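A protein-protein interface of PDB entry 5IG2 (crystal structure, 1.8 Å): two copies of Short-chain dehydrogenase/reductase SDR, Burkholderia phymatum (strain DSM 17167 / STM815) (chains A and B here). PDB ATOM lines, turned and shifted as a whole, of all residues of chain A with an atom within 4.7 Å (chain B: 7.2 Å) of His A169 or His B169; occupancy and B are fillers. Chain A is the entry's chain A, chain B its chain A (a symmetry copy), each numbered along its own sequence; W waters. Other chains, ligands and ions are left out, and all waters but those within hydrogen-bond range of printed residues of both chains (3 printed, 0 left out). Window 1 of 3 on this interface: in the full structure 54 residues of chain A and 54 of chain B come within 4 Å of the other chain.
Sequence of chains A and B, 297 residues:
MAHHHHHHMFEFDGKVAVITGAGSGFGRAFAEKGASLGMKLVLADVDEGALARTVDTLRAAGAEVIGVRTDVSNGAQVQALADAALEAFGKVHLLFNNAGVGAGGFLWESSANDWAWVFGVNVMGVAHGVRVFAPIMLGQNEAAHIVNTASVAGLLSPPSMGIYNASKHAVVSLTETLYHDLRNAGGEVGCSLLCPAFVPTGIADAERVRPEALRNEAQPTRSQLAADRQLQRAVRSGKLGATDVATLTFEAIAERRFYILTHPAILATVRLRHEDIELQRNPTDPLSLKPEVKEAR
Of the 27 printed residues of chain B, 12 touch a printed residue of chain A.
Hydrophobic or aromatic side chains of chain B within 4 Å of the printed part of chain A: Ala B166, His B169, Ala B170, Val B172 and Leu B174.
Along chain B the printed residues that touch a printed residue of chain A span positions 156 to 273.
Among the printed residues, Asp or Glu carboxylates within 4 Å of a Lys or Arg side-chain nitrogen of the other chain: Arg A273 with Glu B176.
Among the printed residues, merely in contact across the chains: Leu A156 with Ser B173, Ser A157 with Thr B177, Asn A165 with Ser B173, Ala A166 with Ala B170, Ala A166 with Ser B173, Ala A166 with Leu B174, His A169 with His B169, Ala A170 with Ala B166, Val A172 with Arg B273, Ser A173 with Leu B156, Ser A173 with Asn B165, Ser A173 with Ala B166 and Arg A273 with Val B172.
A ring nitrogen (ND1) of His B169 lies within hydrogen-bond range of the backbone carbonyl oxygen (O) of Gly B154 (3.3 Å).
The side-chain amide nitrogen of Asn B165 lies within hydrogen-bond range of the backbone carbonyl oxygen of Pro B158, 2.9 Å away.
O of Ala A153 lies close to NE2 of His A169, 3.2 Å away.
His B169 touches two residues of chain A.
Printed residues of chain A within 4 Å of Ser B173: Leu A156, Ser A157, Asn A165, Ala A166 and His A169.
Printed residues of chain A within 4 Å of Asn B165: Ser A173 (3.3 Å).
Of the printed residues of chain A, Ala B170 touches Ala A166.
Thr B175 touches none of the printed residues of chain A.
Val B171 touches none of the printed residues of chain A.
The nearest residue of chain B that does not touch His A169 is Ala B170 (4.4 Å).
The side-chain hydroxyl (OG) of Ser B173 is in hydrogen-bond range of the side-chain hydroxyl (OG) of Ser A157, 2.7 Å away.
NE2 of His A169 sits close to OG of Ser B173 (3.2 Å).
The side-chain hydroxyl (OG) of Ser A173 lies close to a ring nitrogen (NE2) of His B169, at 3.2 Å.
The side-chain carboxylate (OE2) of Glu B176 sits at hydrogen-bond distance from the side-chain hydroxyl (OG) of Ser A157.
The guanidinium group (NE) of Arg A273 is in salt-bridge range of the side-chain carboxylate (OE2) of Glu B176 (2.7 Å).
The side-chain hydroxyl of Ser A173 sits at hydrogen-bond distance from the side-chain hydroxyl of Ser B157, 2.7 Å away.
ND2 of Asn A165 lies within hydrogen-bond range of OG1 of Thr B177.
Leu A156 touches Ser B173, and with the chains exchanged Ser A173 touches Leu B156.
Ser A157 touches Ser B173, and with the chains exchanged Ser A173 touches Ser B157.
Ala A166 touches Ser B173, and with the chains exchanged Ser A173 touches Ala B166.
Val A172 touches Arg B273, and with the chains exchanged Arg A273 touches Val B172.
15 positions are printed for both chains.
Water W2 bridges a ring nitrogen (ND1) of His A169 (2.7 Å) and a ring nitrogen (ND1) of His B169 (2.7 Å).
Water W3 bridges O of Gly A154 (3.0 Å) and NH2 of Arg B273 (3.0 Å).
Water W1 lies within hydrogen-bond range of the backbone carbonyl oxygen of Gly B154 and the guanidinium group of Arg A273.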
ATOM      1  N   ALA A 153      24.340  15.225 -11.190  1.00  0.00           N
ATOM      2  CA  ALA A 153      23.836  14.115 -10.395  1.00  0.00           C
ATOM      3  C   ALA A 153      23.758  12.825 -11.194  1.00  0.00           C
ATOM      4  O   ALA A 153      23.534  11.767 -10.598  1.00  0.00           O
ATOM      5  CB  ALA A 153      22.462  14.461  -9.813  1.00  0.00           C
ATOM      6  N   GLY A 154      23.918  12.887 -12.520  1.00  0.00           N
ATOM      7  CA  GLY A 154      24.132  11.690 -13.313  1.00  0.00           C
ATOM      8  C   GLY A 154      25.569  11.218 -13.370  1.00  0.00           C
ATOM      9  O   GLY A 154      25.846  10.165 -13.951  1.00  0.00           O
ATOM     10  N   LEU A 155      26.493  11.988 -12.793  1.00  0.00           N
ATOM     11  CA  LEU A 155      27.901  11.629 -12.713  1.00  0.00           C
ATOM     12  C   LEU A 155      28.374  11.448 -11.285  1.00  0.00           C
ATOM     13  O   LEU A 155      29.482  10.944 -11.077  1.00  0.00           O
ATOM     14  CB  LEU A 155      28.768  12.704 -13.393  1.00  0.00           C
ATOM     15  CG  LEU A 155      28.306  13.184 -14.776  1.00  0.00           C
ATOM     16  CD1 LEU A 155      29.072  14.451 -15.176  1.00  0.00           C
ATOM     17  CD2 LEU A 155      28.469  12.101 -15.841  1.00  0.00           C
ATOM     18  N   LEU A 156      27.570  11.852 -10.304  1.00  0.00           N
ATOM     19  CA  LEU A 156      27.896  11.808  -8.887  1.00  0.00           C
ATOM     20  C   LEU A 156      26.729  11.165  -8.154  1.00  0.00           C
ATOM     21  O   LEU A 156      25.641  10.987  -8.711  1.00  0.00           O
ATOM     22  CB  LEU A 156      28.156  13.217  -8.327  1.00  0.00           C
ATOM     23  CG  LEU A 156      29.262  14.062  -8.966  1.00  0.00           C
ATOM     24  CD1 LEU A 156      29.191  15.489  -8.454  1.00  0.00           C
ATOM     25  CD2 LEU A 156      30.625  13.461  -8.673  1.00  0.00           C
ATOM     26  N   SER A 157      26.946  10.822  -6.892  1.00  0.00           N
ATOM     27  CA  SER A 157      25.895  10.248  -6.056  1.00  0.00           C
ATOM     28  C   SER A 157      25.886  10.965  -4.715  1.00  0.00           C
ATOM     29  O   SER A 157      26.357  10.426  -3.703  1.00  0.00           O
ATOM     30  CB  SER A 157      26.089   8.739  -5.898  1.00  0.00           C
ATOM     31  OG  SER A 157      25.940   8.110  -7.160  1.00  0.00           O
ATOM     32  N   ASN A 165      19.379  10.978  -8.306  1.00  0.00           N
ATOM     33  CA  ASN A 165      20.673  10.505  -8.787  1.00  0.00           C
ATOM     34  C   ASN A 165      20.512   9.317  -9.725  1.00  0.00           C
ATOM     35  O   ASN A 165      21.023   9.322 -10.851  1.00  0.00           O
ATOM     36  CB  ASN A 165      21.554  10.097  -7.601  1.00  0.00           C
ATOM     37  CG  ASN A 165      21.855  11.239  -6.660  1.00  0.00           C
ATOM     38  OD1 ASN A 165      21.702  12.417  -7.002  1.00  0.00           O
ATOM     39  ND2 ASN A 165      22.318  10.895  -5.458  1.00  0.00           N
ATOM     40  N   ALA A 166      19.804   8.281  -9.264  1.00  0.00           N
ATOM     41  CA  ALA A 166      19.653   7.068 -10.063  1.00  0.00           C
ATOM     42  C   ALA A 166      18.990   7.368 -11.398  1.00  0.00           C
ATOM     43  O   ALA A 166      19.395   6.824 -12.434  1.00  0.00           O
ATOM     44  CB  ALA A 166      18.844   6.015  -9.299  1.00  0.00           C
ATOM     45  N   SER A 167      17.960   8.221 -11.396  1.00  0.00           N
ATOM     46  CA  SER A 167      17.303   8.550 -12.659  1.00  0.00           C
ATOM     47  C   SER A 167      18.275   9.246 -13.602  1.00  0.00           C
ATOM     48  O   SER A 167      18.261   9.003 -14.815  1.00  0.00           O
ATOM     49  CB  SER A 167      16.072   9.426 -12.418  1.00  0.00           C
ATOM     50  OG  SER A 167      16.450  10.748 -12.062  1.00  0.00           O
ATOM     51  N   LYS A 168      19.141  10.102 -13.063  1.00  0.00           N
ATOM     52  CA  LYS A 168      20.050  10.842 -13.931  1.00  0.00           C
ATOM     53  C   LYS A 168      21.216   9.977 -14.410  1.00  0.00           C
ATOM     54  O   LYS A 168      21.679  10.145 -15.544  1.00  0.00           O
ATOM     55  CB  LYS A 168      20.545  12.104 -13.215  1.00  0.00           C
ATOM     56  CG  LYS A 168      19.437  13.137 -12.978  1.00  0.00           C
ATOM     57  CD  LYS A 168      18.725  13.489 -14.293  1.00  0.00           C
ATOM     58  CE  LYS A 168      17.836  14.707 -14.125  1.00  0.00           C
ATOM     59  NZ  LYS A 168      17.299  15.203 -15.438  1.00  0.00           N
ATOM     60  N   HIS A 169      21.693   9.042 -13.584  1.00  0.00           N
ATOM     61  CA  HIS A 169      22.661   8.074 -14.084  1.00  0.00           C
ATOM     62  C   HIS A 169      22.071   7.238 -15.211  1.00  0.00           C
ATOM     63  O   HIS A 169      22.765   6.921 -16.184  1.00  0.00           O
ATOM     64  CB  HIS A 169      23.159   7.175 -12.952  1.00  0.00           C
ATOM     65  CG  HIS A 169      24.181   7.835 -12.083  1.00  0.00           C
ATOM     66  ND1 HIS A 169      25.507   7.457 -12.074  1.00  0.00           N
ATOM     67  CD2 HIS A 169      24.077   8.872 -11.215  1.00  0.00           C
ATOM     68  CE1 HIS A 169      26.172   8.222 -11.223  1.00  0.00           C
ATOM     69  NE2 HIS A 169      25.327   9.089 -10.690  1.00  0.00           N
ATOM     70  N   ALA A 170      20.791   6.866 -15.099  1.00  0.00           N
ATOM     71  CA  ALA A 170      20.143   6.151 -16.194  1.00  0.00           C
ATOM     72  C   ALA A 170      20.145   6.989 -17.471  1.00  0.00           C
ATOM     73  O   ALA A 170      20.433   6.474 -18.558  1.00  0.00           O
ATOM     74  CB  ALA A 170      18.723   5.754 -15.796  1.00  0.00           C
ATOM     75  N   VAL A 171      19.856   8.292 -17.361  1.00  0.00           N
ATOM     76  CA  VAL A 171      19.860   9.142 -18.551  1.00  0.00           C
ATOM     77  C   VAL A 171      21.257   9.222 -19.150  1.00  0.00           C
ATOM     78  O   VAL A 171      21.430   9.133 -20.373  1.00  0.00           O
ATOM     79  CB  VAL A 171      19.310  10.537 -18.222  1.00  0.00           C
ATOM     80  CG1 VAL A 171      19.435  11.465 -19.448  1.00  0.00           C
ATOM     81  CG2 VAL A 171      17.863  10.417 -17.772  1.00  0.00           C
ATOM     82  N   VAL A 172      22.274   9.391 -18.298  1.00  0.00           N
ATOM     83  CA  VAL A 172      23.657   9.393 -18.776  1.00  0.00           C
ATOM     84  C   VAL A 172      23.930   8.155 -19.622  1.00  0.00           C
ATOM     85  O   VAL A 172      24.350   8.252 -20.783  1.00  0.00           O
ATOM     86  CB  VAL A 172      24.636   9.479 -17.595  1.00  0.00           C
ATOM     87  CG1 VAL A 172      26.054   9.113 -18.068  1.00  0.00           C
ATOM     88  CG2 VAL A 172      24.595  10.865 -16.992  1.00  0.00           C
ATOM     89  N   SER A 173      23.670   6.972 -19.060  1.00  0.00           N
ATOM     90  CA  SER A 173      24.061   5.749 -19.751  1.00  0.00           C
ATOM     91  C   SER A 173      23.231   5.512 -21.006  1.00  0.00           C
ATOM     92  O   SER A 173      23.776   5.121 -22.046  1.00  0.00           O
ATOM     93  CB  SER A 173      23.957   4.540 -18.823  1.00  0.00           C
ATOM     94  OG  SER A 173      24.466   3.397 -19.498  1.00  0.00           O
ATOM     95  N   ARG A 273      34.866  10.324  -7.479  1.00  0.00           N
ATOM     96  CA  ARG A 273      33.993   9.161  -7.580  1.00  0.00           C
ATOM     97  C   ARG A 273      34.598   8.113  -8.504  1.00  0.00           C
ATOM     98  O   ARG A 273      34.582   6.915  -8.192  1.00  0.00           O
ATOM     99  CB  ARG A 273      32.597   9.582  -8.067  1.00  0.00           C
ATOM    100  CG  ARG A 273      31.669   8.398  -8.358  1.00  0.00           C
ATOM    101  CD  ARG A 273      30.230   8.756  -8.799  1.00  0.00           C
ATOM    102  NE  ARG A 273      29.537   7.498  -9.058  1.00  0.00           N
ATOM    103  CZ  ARG A 273      29.501   6.871 -10.231  1.00  0.00           C
ATOM    104  NH1 ARG A 273      30.049   7.413 -11.314  1.00  0.00           N
ATOM    105  NH2 ARG A 273      28.907   5.691 -10.322  1.00  0.00           N
ATOM    106  N   VAL B 123      15.355  -1.891 -11.474  1.00  0.00           N
ATOM    107  CA  VAL B 123      15.402  -0.702 -10.627  1.00  0.00           C
ATOM    108  C   VAL B 123      14.327  -0.747  -9.536  1.00  0.00           C
ATOM    109  O   VAL B 123      14.636  -0.664  -8.342  1.00  0.00           O
ATOM    110  CB  VAL B 123      15.305   0.598 -11.458  1.00  0.00           C
ATOM    111  CG1 VAL B 123      15.308   1.819 -10.530  1.00  0.00           C
ATOM    112  CG2 VAL B 123      16.478   0.699 -12.458  1.00  0.00           C
ATOM    113  N   ALA B 150      24.233  -4.967  -9.481  1.00  0.00           N
ATOM    114  CA  ALA B 150      24.220  -4.172 -10.699  1.00  0.00           C
ATOM    115  C   ALA B 150      24.827  -5.022 -11.804  1.00  0.00           C
ATOM    116  O   ALA B 150      24.294  -6.088 -12.126  1.00  0.00           O
ATOM    117  CB  ALA B 150      24.978  -2.856 -10.514  1.00  0.00           C
ATOM    118  N   SER B 151      25.960  -4.577 -12.349  1.00  0.00           N
ATOM    119  CA  SER B 151      26.656  -5.229 -13.454  1.00  0.00           C
ATOM    120  C   SER B 151      27.800  -4.316 -13.872  1.00  0.00           C
ATOM    121  O   SER B 151      27.775  -3.125 -13.537  1.00  0.00           O
ATOM    122  CB  SER B 151      25.701  -5.475 -14.631  1.00  0.00           C
ATOM    123  OG  SER B 151      26.409  -5.753 -15.813  1.00  0.00           O
ATOM    124  N   VAL B 152      28.799  -4.825 -14.605  1.00  0.00           N
ATOM    125  CA  VAL B 152      29.740  -3.883 -15.207  1.00  0.00           C
ATOM    126  C   VAL B 152      29.009  -2.987 -16.187  1.00  0.00           C
ATOM    127  O   VAL B 152      29.492  -1.893 -16.510  1.00  0.00           O
ATOM    128  CB  VAL B 152      30.937  -4.578 -15.893  1.00  0.00           C
ATOM    129  CG1 VAL B 152      31.730  -5.416 -14.881  1.00  0.00           C
ATOM    130  CG2 VAL B 152      30.480  -5.388 -17.085  1.00  0.00           C
ATOM    131  N   ALA B 153      27.834  -3.419 -16.657  1.00  0.00           N
ATOM    132  CA  ALA B 153      26.987  -2.557 -17.469  1.00  0.00           C
ATOM    133  C   ALA B 153      26.436  -1.383 -16.677  1.00  0.00           C
ATOM    134  O   ALA B 153      25.865  -0.472 -17.283  1.00  0.00           O
ATOM    135  CB  ALA B 153      25.840  -3.367 -18.081  1.00  0.00           C
ATOM    136  N   GLY B 154      26.577  -1.390 -15.348  1.00  0.00           N
ATOM    137  CA  GLY B 154      26.333  -0.198 -14.555  1.00  0.00           C
ATOM    138  C   GLY B 154      27.506   0.753 -14.466  1.00  0.00           C
ATOM    139  O   GLY B 154      27.377   1.833 -13.883  1.00  0.00           O
ATOM    140  N   LEU B 155      28.656   0.365 -15.018  1.00  0.00           N
ATOM    141  CA  LEU B 155      29.846   1.202 -15.067  1.00  0.00           C
ATOM    142  C   LEU B 155      30.258   1.545 -16.484  1.00  0.00           C
ATOM    143  O   LEU B 155      31.119   2.411 -16.668  1.00  0.00           O
ATOM    144  CB  LEU B 155      31.023   0.502 -14.362  1.00  0.00           C
ATOM    145  CG  LEU B 155      30.729  -0.117 -12.988  1.00  0.00           C
ATOM    146  CD1 LEU B 155      31.887  -1.031 -12.565  1.00  0.00           C
ATOM    147  CD2 LEU B 155      30.472   0.949 -11.924  1.00  0.00           C
ATOM    148  N   LEU B 156      29.673   0.885 -17.482  1.00  0.00           N
ATOM    149  CA  LEU B 156      29.995   1.049 -18.891  1.00  0.00           C
ATOM    150  C   LEU B 156      28.693   1.237 -19.654  1.00  0.00           C
ATOM    151  O   LEU B 156      27.600   1.015 -19.124  1.00  0.00           O
ATOM    152  CB  LEU B 156      30.753  -0.173 -19.438  1.00  0.00           C
ATOM    153  CG  LEU B 156      32.071  -0.572 -18.770  1.00  0.00           C
ATOM    154  CD1 LEU B 156      32.525  -1.929 -19.277  1.00  0.00           C
ATOM    155  CD2 LEU B 156      33.138   0.475 -19.033  1.00  0.00           C
ATOM    156  N   SER B 157      28.804   1.641 -20.912  1.00  0.00           N
ATOM    157  CA  SER B 157      27.637   1.807 -21.775  1.00  0.00           C
ATOM    158  C   SER B 157      27.916   1.140 -23.113  1.00  0.00           C
ATOM    159  O   SER B 157      28.188   1.816 -24.116  1.00  0.00           O
ATOM    160  CB  SER B 157      27.286   3.288 -21.935  1.00  0.00           C
ATOM    161  OG  SER B 157      26.893   3.817 -20.680  1.00  0.00           O
ATOM    162  N   PRO B 158      27.856  -0.195 -23.166  1.00  0.00           N
ATOM    163  CA  PRO B 158      28.142  -0.884 -24.422  1.00  0.00           C
ATOM    164  C   PRO B 158      26.988  -0.736 -25.397  1.00  0.00           C
ATOM    165  O   PRO B 158      25.817  -0.631 -24.992  1.00  0.00           O
ATOM    166  CB  PRO B 158      28.324  -2.351 -23.993  1.00  0.00           C
ATOM    167  CG  PRO B 158      28.177  -2.381 -22.531  1.00  0.00           C
ATOM    168  CD  PRO B 158      27.535  -1.132 -22.083  1.00  0.00           C
ATOM    169  N   GLY B 162      21.207  -0.426 -24.272  1.00  0.00           N
ATOM    170  CA  GLY B 162      20.990   0.834 -23.563  1.00  0.00           C
ATOM    171  C   GLY B 162      19.975   0.772 -22.436  1.00  0.00           C
ATOM    172  O   GLY B 162      20.133   1.454 -21.423  1.00  0.00           O
ATOM    173  N   ILE B 163      18.900  -0.006 -22.601  1.00  0.00           N
ATOM    174  CA  ILE B 163      17.902  -0.080 -21.532  1.00  0.00           C
ATOM    175  C   ILE B 163      18.488  -0.791 -20.327  1.00  0.00           C
ATOM    176  O   ILE B 163      18.353  -0.336 -19.181  1.00  0.00           O
ATOM    177  CB  ILE B 163      16.622  -0.781 -22.010  1.00  0.00           C
ATOM    178  CG1 ILE B 163      15.984  -0.014 -23.170  1.00  0.00           C
ATOM    179  CG2 ILE B 163      15.629  -0.889 -20.850  1.00  0.00           C
ATOM    180  CD1 ILE B 163      14.686  -0.650 -23.632  1.00  0.00           C
ATOM    181  N   TYR B 164      19.153  -1.922 -20.577  1.00  0.00           N
ATOM    182  CA  TYR B 164      19.818  -2.658 -19.510  1.00  0.00           C
ATOM    183  C   TYR B 164      20.888  -1.800 -18.857  1.00  0.00           C
ATOM    184  O   TYR B 164      20.940  -1.678 -17.628  1.00  0.00           O
ATOM    185  CB  TYR B 164      20.428  -3.935 -20.091  1.00  0.00           C
ATOM    186  CG  TYR B 164      21.060  -4.853 -19.075  1.00  0.00           C
ATOM    187  CD1 TYR B 164      20.276  -5.650 -18.262  1.00  0.00           C
ATOM    188  CD2 TYR B 164      22.443  -4.936 -18.943  1.00  0.00           C
ATOM    189  CE1 TYR B 164      20.842  -6.499 -17.339  1.00  0.00           C
ATOM    190  CE2 TYR B 164      23.024  -5.793 -18.017  1.00  0.00           C
ATOM    191  CZ  TYR B 164      22.214  -6.572 -17.220  1.00  0.00           C
ATOM    192  OH  TYR B 164      22.747  -7.436 -16.283  1.00  0.00           O
ATOM    193  N   ASN B 165      21.756  -1.201 -19.676  1.00  0.00           N
ATOM    194  CA  ASN B 165      22.786  -0.301 -19.167  1.00  0.00           C
ATOM    195  C   ASN B 165      22.190   0.747 -18.237  1.00  0.00           C
ATOM    196  O   ASN B 165      22.643   0.920 -17.100  1.00  0.00           O
ATOM    197  CB  ASN B 165      23.492   0.398 -20.333  1.00  0.00           C
ATOM    198  CG  ASN B 165      24.201  -0.558 -21.262  1.00  0.00           C
ATOM    199  OD1 ASN B 165      24.469  -1.715 -20.918  1.00  0.00           O
ATOM    200  ND2 ASN B 165      24.540  -0.066 -22.454  1.00  0.00           N
ATOM    201  N   ALA B 166      21.171   1.466 -18.720  1.00  0.00           N
ATOM    202  CA  ALA B 166      20.580   2.543 -17.930  1.00  0.00           C
ATOM    203  C   ALA B 166      20.036   2.021 -16.610  1.00  0.00           C
ATOM    204  O   ALA B 166      20.197   2.669 -15.567  1.00  0.00           O
ATOM    205  CB  ALA B 166      19.468   3.243 -18.717  1.00  0.00           C
ATOM    206  N   SER B 167      19.378   0.857 -16.632  1.00  0.00           N
ATOM    207  CA  SER B 167      18.851   0.311 -15.383  1.00  0.00           C
ATOM    208  C   SER B 167      19.984   0.002 -14.415  1.00  0.00           C
ATOM    209  O   SER B 167      19.856   0.218 -13.204  1.00  0.00           O
ATOM    210  CB  SER B 167      18.017  -0.945 -15.649  1.00  0.00           C
ATOM    211  OG  SER B 167      18.849  -2.044 -15.991  1.00  0.00           O
ATOM    212  N   LYS B 168      21.110  -0.488 -14.930  1.00  0.00           N
ATOM    213  CA  LYS B 168      22.202  -0.860 -14.037  1.00  0.00           C
ATOM    214  C   LYS B 168      22.973   0.360 -13.535  1.00  0.00           C
ATOM    215  O   LYS B 168      23.439   0.363 -12.390  1.00  0.00           O
ATOM    216  CB  LYS B 168      23.131  -1.860 -14.736  1.00  0.00           C
ATOM    217  CG  LYS B 168      22.468  -3.219 -14.994  1.00  0.00           C
ATOM    218  CD  LYS B 168      21.898  -3.807 -13.695  1.00  0.00           C
ATOM    219  CE  LYS B 168      21.503  -5.260 -13.879  1.00  0.00           C
ATOM    220  NZ  LYS B 168      21.147  -5.921 -12.576  1.00  0.00           N
ATOM    221  N   HIS B 169      23.106   1.408 -14.354  1.00  0.00           N
ATOM    222  CA  HIS B 169      23.654   2.655 -13.835  1.00  0.00           C
ATOM    223  C   HIS B 169      22.779   3.221 -12.726  1.00  0.00           C
ATOM    224  O   HIS B 169      23.292   3.760 -11.738  1.00  0.00           O
ATOM    225  CB  HIS B 169      23.827   3.677 -14.958  1.00  0.00           C
ATOM    226  CG  HIS B 169      25.037   3.427 -15.801  1.00  0.00           C
ATOM    227  ND1 HIS B 169      26.141   4.252 -15.780  1.00  0.00           N
ATOM    228  CD2 HIS B 169      25.328   2.425 -16.667  1.00  0.00           C
ATOM    229  CE1 HIS B 169      27.055   3.777 -16.612  1.00  0.00           C
ATOM    230  NE2 HIS B 169      26.586   2.669 -17.161  1.00  0.00           N
ATOM    231  N   ALA B 170      21.453   3.115 -12.869  1.00  0.00           N
ATOM    232  CA  ALA B 170      20.568   3.548 -11.793  1.00  0.00           C
ATOM    233  C   ALA B 170      20.838   2.759 -10.513  1.00  0.00           C
ATOM    234  O   ALA B 170      20.898   3.339  -9.422  1.00  0.00           O
ATOM    235  CB  ALA B 170      19.109   3.415 -12.226  1.00  0.00           C
ATOM    236  N   VAL B 171      21.034   1.440 -10.623  1.00  0.00           N
ATOM    237  CA  VAL B 171      21.312   0.641  -9.430  1.00  0.00           C
ATOM    238  C   VAL B 171      22.631   1.061  -8.798  1.00  0.00           C
ATOM    239  O   VAL B 171      22.733   1.200  -7.572  1.00  0.00           O
ATOM    240  CB  VAL B 171      21.301  -0.857  -9.766  1.00  0.00           C
ATOM    241  CG1 VAL B 171      21.719  -1.685  -8.533  1.00  0.00           C
ATOM    242  CG2 VAL B 171      19.918  -1.257 -10.251  1.00  0.00           C
ATOM    243  N   VAL B 172      23.662   1.268  -9.625  1.00  0.00           N
ATOM    244  CA  VAL B 172      24.944   1.756  -9.115  1.00  0.00           C
ATOM    245  C   VAL B 172      24.738   3.006  -8.268  1.00  0.00           C
ATOM    246  O   VAL B 172      25.138   3.060  -7.097  1.00  0.00           O
ATOM    247  CB  VAL B 172      25.916   2.028 -10.272  1.00  0.00           C
ATOM    248  CG1 VAL B 172      27.100   2.873  -9.768  1.00  0.00           C
ATOM    249  CG2 VAL B 172      26.385   0.722 -10.870  1.00  0.00           C
ATOM    250  N   SER B 173      24.087   4.022  -8.841  1.00  0.00           N
ATOM    251  CA  SER B 173      24.002   5.301  -8.146  1.00  0.00           C
ATOM    252  C   SER B 173      23.113   5.222  -6.912  1.00  0.00           C
ATOM    253  O   SER B 173      23.459   5.777  -5.862  1.00  0.00           O
ATOM    254  CB  SER B 173      23.497   6.398  -9.082  1.00  0.00           C
ATOM    255  OG  SER B 173      23.550   7.644  -8.400  1.00  0.00           O
ATOM    256  N   LEU B 174      21.951   4.572  -7.013  1.00  0.00           N
ATOM    257  CA  LEU B 174      21.106   4.502  -5.824  1.00  0.00           C
ATOM    258  C   LEU B 174      21.823   3.770  -4.699  1.00  0.00           C
ATOM    259  O   LEU B 174      21.647   4.120  -3.529  1.00  0.00           O
ATOM    260  CB  LEU B 174      19.756   3.847  -6.136  1.00  0.00           C
ATOM    261  CG  LEU B 174      19.628   2.326  -6.251  1.00  0.00           C
ATOM    262  CD1 LEU B 174      19.450   1.633  -4.885  1.00  0.00           C
ATOM    263  CD2 LEU B 174      18.459   1.996  -7.183  1.00  0.00           C
ATOM    264  N   THR B 175      22.658   2.780  -5.036  1.00  0.00           N
ATOM    265  CA  THR B 175      23.360   2.020  -4.007  1.00  0.00           C
ATOM    266  C   THR B 175      24.505   2.836  -3.411  1.00  0.00           C
ATOM    267  O   THR B 175      24.728   2.806  -2.194  1.00  0.00           O
ATOM    268  CB  THR B 175      23.861   0.684  -4.574  1.00  0.00           C
ATOM    269  OG1 THR B 175      22.769  -0.035  -5.167  1.00  0.00           O
ATOM    270  CG2 THR B 175      24.443  -0.202  -3.462  1.00  0.00           C
ATOM    271  N   GLU B 176      25.226   3.588  -4.244  1.00  0.00           N
ATOM    272  CA  GLU B 176      26.201   4.542  -3.717  1.00  0.00           C
ATOM    273  C   GLU B 176      25.533   5.535  -2.773  1.00  0.00           C
ATOM    274  O   GLU B 176      26.038   5.807  -1.676  1.00  0.00           O
ATOM    275  CB  GLU B 176      26.900   5.279  -4.866  1.00  0.00           C
ATOM    276  CG  GLU B 176      27.806   4.386  -5.712  1.00  0.00           C
ATOM    277  CD  GLU B 176      28.393   5.111  -6.921  1.00  0.00           C
ATOM    278  OE1 GLU B 176      29.348   4.572  -7.527  1.00  0.00           O
ATOM    279  OE2 GLU B 176      27.906   6.214  -7.262  1.00  0.00           O
ATOM    280  N   THR B 177      24.389   6.092  -3.181  1.00  0.00           N
ATOM    281  CA  THR B 177      23.701   7.040  -2.310  1.00  0.00           C
ATOM    282  C   THR B 177      23.265   6.368  -1.017  1.00  0.00           C
ATOM    283  O   THR B 177      23.380   6.955   0.068  1.00  0.00           O
ATOM    284  CB  THR B 177      22.487   7.646  -3.011  1.00  0.00           C
ATOM    285  OG1 THR B 177      22.871   8.149  -4.304  1.00  0.00           O
ATOM    286  CG2 THR B 177      21.925   8.796  -2.163  1.00  0.00           C
ATOM    287  N   ARG B 273      36.014   4.920 -20.141  1.00  0.00           N
ATOM    288  CA  ARG B 273      34.782   5.696 -20.066  1.00  0.00           C
ATOM    289  C   ARG B 273      34.952   6.887 -19.132  1.00  0.00           C
ATOM    290  O   ARG B 273      34.519   8.002 -19.450  1.00  0.00           O
ATOM    291  CB  ARG B 273      33.615   4.804 -19.610  1.00  0.00           C
ATOM    292  CG  ARG B 273      32.321   5.580 -19.346  1.00  0.00           C
ATOM    293  CD  ARG B 273      31.093   4.732 -18.937  1.00  0.00           C
ATOM    294  NE  ARG B 273      29.992   5.660 -18.700  1.00  0.00           N
ATOM    295  CZ  ARG B 273      29.708   6.228 -17.531  1.00  0.00           C
ATOM    296  NH1 ARG B 273      30.387   5.912 -16.433  1.00  0.00           N
ATOM    297  NH2 ARG B 273      28.732   7.119 -17.459  1.00  0.00           N
HETATM  298  O   HOH W   1      28.824   4.255 -12.971  1.00  0.00           O
HETATM  299  O   HOH W   2      26.922   6.056 -13.914  1.00  0.00           O
HETATM  300  O   HOH W   3      28.081   8.421 -14.819  1.00  0.00           O
